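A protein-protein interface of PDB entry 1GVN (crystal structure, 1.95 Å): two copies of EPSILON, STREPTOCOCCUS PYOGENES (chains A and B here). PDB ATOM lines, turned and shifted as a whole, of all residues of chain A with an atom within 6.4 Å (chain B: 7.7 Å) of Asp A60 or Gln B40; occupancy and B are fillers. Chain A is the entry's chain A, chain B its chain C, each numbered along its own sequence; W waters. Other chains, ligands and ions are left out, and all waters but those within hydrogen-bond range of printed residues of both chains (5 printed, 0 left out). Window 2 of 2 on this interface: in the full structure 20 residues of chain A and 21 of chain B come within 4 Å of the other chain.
No position is printed for both chains.
Of the 10 printed residues of chain A, 4 touch a printed residue of chain B. Among the printed residues, 8 pairs touch across the chains.
The side-chain amide oxygen (OD1) of Asn A57 sits close to the backbone NH (N) of Phe A59 (3.1 Å). The backbone NH (N) of Gln B40 is in hydrogen-bond range of the side-chain carboxylate (OD1) of Asp B38. The side-chain amide nitrogen (ND2) of Asn B45 lies within hydrogen-bond range of the backbone carbonyl oxygen (O) of Ser B39 (3.2 Å).
Among the printed residues, pairs that only touch across the chains: Val A56 with Asn B45 (3.3 Å), Val A56 with Gln B40 (3.5 Å), Val A56 with Ser B39 (3.7 Å) and Tyr A61 with Leu B41 (3.9 Å).
Of chain B, only Gln B40 (3.2 Å) comes within 4 Å of Asp A60. Of chain A, only Val A56, Asn A57, Asp A60 and Tyr A61 come within 4 Å of Gln B40. Of the printed residues of chain B, Tyr A61 touches Gln B40 (2.6 Å), Leu B41 (3.9 Å) and Leu B42 (3.4 Å). Printed residues of chain B within 4 Å of Val A56: Ser B39, Gln B40 and Asn B45. The nearest residue of chain B that does not touch Asp A60 is Leu B41 (5.8 Å).
Water W4 bridges OE1 of Gln B40 (2.5 Å) and O of Arg A55 (3.2 Å). Water W3 bridges OE2 of Glu B43 (2.6 Å) and OE2 of Glu A65 (2.9 Å). Water W2 bridges the side-chain carboxylate of Glu A65 (2.6 Å) and the backbone NH of Leu B42 (3.0 Å). Water W1 bridges the side-chain hydroxyl of Ser B39 (2.8 Å) and the guanidinium group of Arg A55 (2.8 Å). Water W5 lies within hydrogen-bond range of O of Arg A55, O of Ser B39 and N of Val A56.
The side-chain amide oxygen (OE1) of Gln B40 lies within hydrogen-bond range of the backbone NH (N) of Asn A57 (2.7 Å). The side-chain carboxylate (OD2) of Asp A60 is in hydrogen-bond range of the side-chain amide nitrogen (NE2) of Gln B40 (3.2 Å). The side-chain hydroxyl of Tyr A61 is in hydrogen-bond range of the backbone carbonyl oxygen of Gln B40, at 2.6 Å. The side-chain hydroxyl of Tyr A61 is in hydrogen-bond range of the backbone NH of Leu B42.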
ATOM      1  N   ILE A  11     -18.808 -33.199  13.185  1.00  0.00           N
ATOM      2  CA  ILE A  11     -19.500 -33.005  11.917  1.00  0.00           C
ATOM      3  C   ILE A  11     -19.957 -34.330  11.305  1.00  0.00           C
ATOM      4  O   ILE A  11     -21.047 -34.414  10.740  1.00  0.00           O
ATOM      5  CB  ILE A  11     -18.605 -32.240  10.913  1.00  0.00           C
ATOM      6  CG1 ILE A  11     -18.436 -30.790  11.392  1.00  0.00           C
ATOM      7  CG2 ILE A  11     -19.211 -32.294   9.511  1.00  0.00           C
ATOM      8  CD1 ILE A  11     -17.541 -29.933  10.521  1.00  0.00           C
ATOM      9  N   ARG A  55     -29.090 -26.247   5.256  1.00  0.00           N
ATOM     10  CA  ARG A  55     -28.434 -25.347   4.310  1.00  0.00           C
ATOM     11  C   ARG A  55     -27.120 -24.760   4.827  1.00  0.00           C
ATOM     12  O   ARG A  55     -26.359 -24.167   4.061  1.00  0.00           O
ATOM     13  CB  ARG A  55     -29.366 -24.195   3.944  1.00  0.00           C
ATOM     14  CG  ARG A  55     -30.581 -24.584   3.126  1.00  0.00           C
ATOM     15  CD  ARG A  55     -31.394 -23.341   2.812  1.00  0.00           C
ATOM     16  NE  ARG A  55     -32.578 -23.628   2.011  1.00  0.00           N
ATOM     17  CZ  ARG A  55     -33.460 -22.707   1.639  1.00  0.00           C
ATOM     18  NH1 ARG A  55     -33.288 -21.442   1.998  1.00  0.00           N
ATOM     19  NH2 ARG A  55     -34.514 -23.048   0.910  1.00  0.00           N
ATOM     20  N   VAL A  56     -26.849 -24.930   6.116  1.00  0.00           N
ATOM     21  CA  VAL A  56     -25.639 -24.366   6.708  1.00  0.00           C
ATOM     22  C   VAL A  56     -24.345 -25.099   6.379  1.00  0.00           C
ATOM     23  O   VAL A  56     -24.345 -26.304   6.122  1.00  0.00           O
ATOM     24  CB  VAL A  56     -25.756 -24.292   8.245  1.00  0.00           C
ATOM     25  CG1 VAL A  56     -27.001 -23.509   8.636  1.00  0.00           C
ATOM     26  CG2 VAL A  56     -25.802 -25.684   8.826  1.00  0.00           C
ATOM     27  N   ASN A  57     -23.241 -24.356   6.388  1.00  0.00           N
ATOM     28  CA  ASN A  57     -21.923 -24.941   6.138  1.00  0.00           C
ATOM     29  C   ASN A  57     -21.264 -25.184   7.486  1.00  0.00           C
ATOM     30  O   ASN A  57     -20.729 -24.258   8.100  1.00  0.00           O
ATOM     31  CB  ASN A  57     -21.043 -24.006   5.315  1.00  0.00           C
ATOM     32  CG  ASN A  57     -19.588 -24.446   5.316  1.00  0.00           C
ATOM     33  OD1 ASN A  57     -19.297 -25.642   5.320  1.00  0.00           O
ATOM     34  ND2 ASN A  57     -18.671 -23.487   5.312  1.00  0.00           N
ATOM     35  N   LEU A  58     -21.298 -26.435   7.935  1.00  0.00           N
ATOM     36  CA  LEU A  58     -20.740 -26.803   9.226  1.00  0.00           C
ATOM     37  C   LEU A  58     -19.241 -26.583   9.348  1.00  0.00           C
ATOM     38  O   LEU A  58     -18.722 -26.490  10.455  1.00  0.00           O
ATOM     39  CB  LEU A  58     -21.070 -28.265   9.541  1.00  0.00           C
ATOM     40  CG  LEU A  58     -22.561 -28.622   9.537  1.00  0.00           C
ATOM     41  CD1 LEU A  58     -22.726 -30.126   9.759  1.00  0.00           C
ATOM     42  CD2 LEU A  58     -23.288 -27.829  10.625  1.00  0.00           C
ATOM     43  N   PHE A  59     -18.544 -26.494   8.221  1.00  0.00           N
ATOM     44  CA  PHE A  59     -17.102 -26.296   8.263  1.00  0.00           C
ATOM     45  C   PHE A  59     -16.715 -24.895   8.715  1.00  0.00           C
ATOM     46  O   PHE A  59     -15.548 -24.625   8.997  1.00  0.00           O
ATOM     47  CB  PHE A  59     -16.493 -26.600   6.892  1.00  0.00           C
ATOM     48  CG  PHE A  59     -16.705 -28.017   6.449  1.00  0.00           C
ATOM     49  CD1 PHE A  59     -16.246 -29.072   7.229  1.00  0.00           C
ATOM     50  CD2 PHE A  59     -17.402 -28.298   5.280  1.00  0.00           C
ATOM     51  CE1 PHE A  59     -16.482 -30.393   6.857  1.00  0.00           C
ATOM     52  CE2 PHE A  59     -17.646 -29.610   4.896  1.00  0.00           C
ATOM     53  CZ  PHE A  59     -17.184 -30.663   5.690  1.00  0.00           C
ATOM     54  N   ASP A  60     -17.701 -24.013   8.807  1.00  0.00           N
ATOM     55  CA  ASP A  60     -17.462 -22.634   9.218  1.00  0.00           C
ATOM     56  C   ASP A  60     -17.776 -22.426  10.701  1.00  0.00           C
ATOM     57  O   ASP A  60     -17.530 -21.349  11.250  1.00  0.00           O
ATOM     58  CB  ASP A  60     -18.319 -21.701   8.350  1.00  0.00           C
ATOM     59  CG  ASP A  60     -18.205 -20.242   8.755  1.00  0.00           C
ATOM     60  OD1 ASP A  60     -17.068 -19.724   8.815  1.00  0.00           O
ATOM     61  OD2 ASP A  60     -19.258 -19.612   9.002  1.00  0.00           O
ATOM     62  N   TYR A  61     -18.300 -23.464  11.347  1.00  0.00           N
ATOM     63  CA  TYR A  61     -18.675 -23.391  12.757  1.00  0.00           C
ATOM     64  C   TYR A  61     -17.595 -23.761  13.761  1.00  0.00           C
ATOM     65  O   TYR A  61     -16.737 -24.601  13.496  1.00  0.00           O
ATOM     66  CB  TYR A  61     -19.892 -24.284  13.027  1.00  0.00           C
ATOM     67  CG  TYR A  61     -21.216 -23.737  12.544  1.00  0.00           C
ATOM     68  CD1 TYR A  61     -21.298 -22.502  11.897  1.00  0.00           C
ATOM     69  CD2 TYR A  61     -22.396 -24.446  12.756  1.00  0.00           C
ATOM     70  CE1 TYR A  61     -22.523 -21.990  11.476  1.00  0.00           C
ATOM     71  CE2 TYR A  61     -23.621 -23.943  12.340  1.00  0.00           C
ATOM     72  CZ  TYR A  61     -23.680 -22.715  11.702  1.00  0.00           C
ATOM     73  OH  TYR A  61     -24.898 -22.216  11.293  1.00  0.00           O
ATOM     74  N   SER A  62     -17.661 -23.128  14.928  1.00  0.00           N
ATOM     75  CA  SER A  62     -16.728 -23.408  16.006  1.00  0.00           C
ATOM     76  C   SER A  62     -17.196 -24.721  16.620  1.00  0.00           C
ATOM     77  O   SER A  62     -18.292 -25.198  16.314  1.00  0.00           O
ATOM     78  CB  SER A  62     -16.786 -22.304  17.062  1.00  0.00           C
ATOM     79  OG  SER A  62     -18.072 -22.248  17.666  1.00  0.00           O
ATOM     80  N   GLU A  65     -20.428 -24.222  18.413  1.00  0.00           N
ATOM     81  CA  GLU A  65     -21.572 -24.101  17.521  1.00  0.00           C
ATOM     82  C   GLU A  65     -21.960 -25.474  16.976  1.00  0.00           C
ATOM     83  O   GLU A  65     -23.137 -25.749  16.761  1.00  0.00           O
ATOM     84  CB  GLU A  65     -21.251 -23.145  16.370  1.00  0.00           C
ATOM     85  CG  GLU A  65     -21.089 -21.697  16.807  1.00  0.00           C
ATOM     86  CD  GLU A  65     -20.742 -20.777  15.652  1.00  0.00           C
ATOM     87  OE1 GLU A  65     -19.783 -21.090  14.913  1.00  0.00           O
ATOM     88  OE2 GLU A  65     -21.421 -19.741  15.482  1.00  0.00           O
ATOM     89  N   ASN B  35     -26.600 -10.176  10.768  1.00  0.00           N
ATOM     90  CA  ASN B  35     -27.298  -9.934   9.518  1.00  0.00           C
ATOM     91  C   ASN B  35     -28.505 -10.872   9.462  1.00  0.00           C
ATOM     92  O   ASN B  35     -28.348 -12.079   9.288  1.00  0.00           O
ATOM     93  CB  ASN B  35     -26.375 -10.223   8.335  1.00  0.00           C
ATOM     94  CG  ASN B  35     -26.997  -9.845   7.011  1.00  0.00           C
ATOM     95  OD1 ASN B  35     -28.182 -10.081   6.779  1.00  0.00           O
ATOM     96  ND2 ASN B  35     -26.198  -9.261   6.129  1.00  0.00           N
ATOM     97  N   ASN B  37     -30.299 -11.448   7.242  1.00  0.00           N
ATOM     98  CA  ASN B  37     -30.354 -12.062   5.919  1.00  0.00           C
ATOM     99  C   ASN B  37     -29.244 -13.089   5.709  1.00  0.00           C
ATOM    100  O   ASN B  37     -28.969 -13.489   4.575  1.00  0.00           O
ATOM    101  CB  ASN B  37     -30.243 -10.991   4.826  1.00  0.00           C
ATOM    102  CG  ASN B  37     -31.310  -9.921   4.942  1.00  0.00           C
ATOM    103  OD1 ASN B  37     -32.498 -10.223   5.074  1.00  0.00           O
ATOM    104  ND2 ASN B  37     -30.892  -8.659   4.884  1.00  0.00           N
ATOM    105  N   ASP B  38     -28.600 -13.513   6.790  1.00  0.00           N
ATOM    106  CA  ASP B  38     -27.521 -14.489   6.672  1.00  0.00           C
ATOM    107  C   ASP B  38     -27.859 -15.777   7.408  1.00  0.00           C
ATOM    108  O   ASP B  38     -27.479 -15.966   8.566  1.00  0.00           O
ATOM    109  CB  ASP B  38     -26.215 -13.907   7.214  1.00  0.00           C
ATOM    110  CG  ASP B  38     -25.039 -14.844   7.027  1.00  0.00           C
ATOM    111  OD1 ASP B  38     -25.249 -15.978   6.542  1.00  0.00           O
ATOM    112  OD2 ASP B  38     -23.905 -14.451   7.369  1.00  0.00           O
ATOM    113  N   SER B  39     -28.558 -16.668   6.714  1.00  0.00           N
ATOM    114  CA  SER B  39     -28.976 -17.944   7.277  1.00  0.00           C
ATOM    115  C   SER B  39     -27.839 -18.902   7.630  1.00  0.00           C
ATOM    116  O   SER B  39     -28.090 -19.997   8.130  1.00  0.00           O
ATOM    117  CB  SER B  39     -29.957 -18.632   6.322  1.00  0.00           C
ATOM    118  OG  SER B  39     -29.435 -18.666   5.002  1.00  0.00           O
ATOM    119  N   GLN B  40     -26.596 -18.504   7.368  1.00  0.00           N
ATOM    120  CA  GLN B  40     -25.443 -19.346   7.708  1.00  0.00           C
ATOM    121  C   GLN B  40     -25.148 -19.213   9.197  1.00  0.00           C
ATOM    122  O   GLN B  40     -24.626 -20.135   9.823  1.00  0.00           O
ATOM    123  CB  GLN B  40     -24.210 -18.926   6.892  1.00  0.00           C
ATOM    124  CG  GLN B  40     -22.848 -19.438   7.397  1.00  0.00           C
ATOM    125  CD  GLN B  40     -22.737 -20.958   7.482  1.00  0.00           C
ATOM    126  OE1 GLN B  40     -23.412 -21.691   6.755  1.00  0.00           O
ATOM    127  NE2 GLN B  40     -21.861 -21.436   8.362  1.00  0.00           N
ATOM    128  N   LEU B  41     -25.486 -18.058   9.763  1.00  0.00           N
ATOM    129  CA  LEU B  41     -25.254 -17.811  11.180  1.00  0.00           C
ATOM    130  C   LEU B  41     -26.217 -18.665  12.000  1.00  0.00           C
ATOM    131  O   LEU B  41     -27.420 -18.679  11.744  1.00  0.00           O
ATOM    132  CB  LEU B  41     -25.459 -16.328  11.494  1.00  0.00           C
ATOM    133  CG  LEU B  41     -24.644 -15.345  10.642  1.00  0.00           C
ATOM    134  CD1 LEU B  41     -24.913 -13.930  11.137  1.00  0.00           C
ATOM    135  CD2 LEU B  41     -23.151 -15.665  10.731  1.00  0.00           C
ATOM    136  N   LEU B  42     -25.678 -19.378  12.983  1.00  0.00           N
ATOM    137  CA  LEU B  42     -26.473 -20.266  13.819  1.00  0.00           C
ATOM    138  C   LEU B  42     -27.742 -19.640  14.386  1.00  0.00           C
ATOM    139  O   LEU B  42     -28.817 -20.222  14.279  1.00  0.00           O
ATOM    140  CB  LEU B  42     -25.624 -20.803  14.972  1.00  0.00           C
ATOM    141  CG  LEU B  42     -26.336 -21.773  15.918  1.00  0.00           C
ATOM    142  CD1 LEU B  42     -26.623 -23.066  15.186  1.00  0.00           C
ATOM    143  CD2 LEU B  42     -25.460 -22.045  17.139  1.00  0.00           C
ATOM    144  N   GLU B  43     -27.617 -18.458  14.986  1.00  0.00           N
ATOM    145  CA  GLU B  43     -28.764 -17.787  15.599  1.00  0.00           C
ATOM    146  C   GLU B  43     -29.803 -17.266  14.609  1.00  0.00           C
ATOM    147  O   GLU B  43     -31.001 -17.248  14.911  1.00  0.00           O
ATOM    148  CB  GLU B  43     -28.292 -16.630  16.487  1.00  0.00           C
ATOM    149  CG  GLU B  43     -27.329 -17.035  17.592  1.00  0.00           C
ATOM    150  CD  GLU B  43     -25.894 -17.151  17.115  1.00  0.00           C
ATOM    151  OE1 GLU B  43     -25.636 -16.918  15.917  1.00  0.00           O
ATOM    152  OE2 GLU B  43     -25.022 -17.473  17.946  1.00  0.00           O
ATOM    153  N   VAL B  44     -29.346 -16.825  13.441  1.00  0.00           N
ATOM    154  CA  VAL B  44     -30.252 -16.309  12.422  1.00  0.00           C
ATOM    155  C   VAL B  44     -31.008 -17.478  11.783  1.00  0.00           C
ATOM    156  O   VAL B  44     -32.203 -17.390  11.507  1.00  0.00           O
ATOM    157  CB  VAL B  44     -29.475 -15.521  11.342  1.00  0.00           C
ATOM    158  CG1 VAL B  44     -30.418 -15.074  10.227  1.00  0.00           C
ATOM    159  CG2 VAL B  44     -28.801 -14.309  11.984  1.00  0.00           C
ATOM    160  N   ASN B  45     -30.298 -18.576  11.558  1.00  0.00           N
ATOM    161  CA  ASN B  45     -30.909 -19.762  10.979  1.00  0.00           C
ATOM    162  C   ASN B  45     -32.008 -20.222  11.935  1.00  0.00           C
ATOM    163  O   ASN B  45     -33.109 -20.559  11.512  1.00  0.00           O
ATOM    164  CB  ASN B  45     -29.852 -20.851  10.798  1.00  0.00           C
ATOM    165  CG  ASN B  45     -30.419 -22.123  10.207  1.00  0.00           C
ATOM    166  OD1 ASN B  45     -31.141 -22.862  10.872  1.00  0.00           O
ATOM    167  ND2 ASN B  45     -30.091 -22.385   8.945  1.00  0.00           N
ATOM    168  N   ASN B  48     -34.999 -17.908  11.729  1.00  0.00           N
ATOM    169  CA  ASN B  48     -35.785 -18.170  10.528  1.00  0.00           C
ATOM    170  C   ASN B  48     -36.650 -19.419  10.668  1.00  0.00           C
ATOM    171  O   ASN B  48     -37.759 -19.471  10.142  1.00  0.00           O
ATOM    172  CB  ASN B  48     -34.859 -18.286   9.315  1.00  0.00           C
ATOM    173  CG  ASN B  48     -34.258 -16.949   8.923  1.00  0.00           C
ATOM    174  OD1 ASN B  48     -33.190 -16.889   8.312  1.00  0.00           O
ATOM    175  ND2 ASN B  48     -34.949 -15.868   9.264  1.00  0.00           N
HETATM  176  O   HOH W   1     -31.462 -20.174   3.750  1.00  0.00           O
HETATM  177  O   HOH W   2     -22.810 -18.746  13.476  1.00  0.00           O
HETATM  178  O   HOH W   3     -22.968 -19.069  17.854  1.00  0.00           O
HETATM  179  O   HOH W   4     -24.854 -21.431   4.669  1.00  0.00           O
HETATM  180  O   HOH W   5     -27.478 -21.580   5.446  1.00  0.00           O
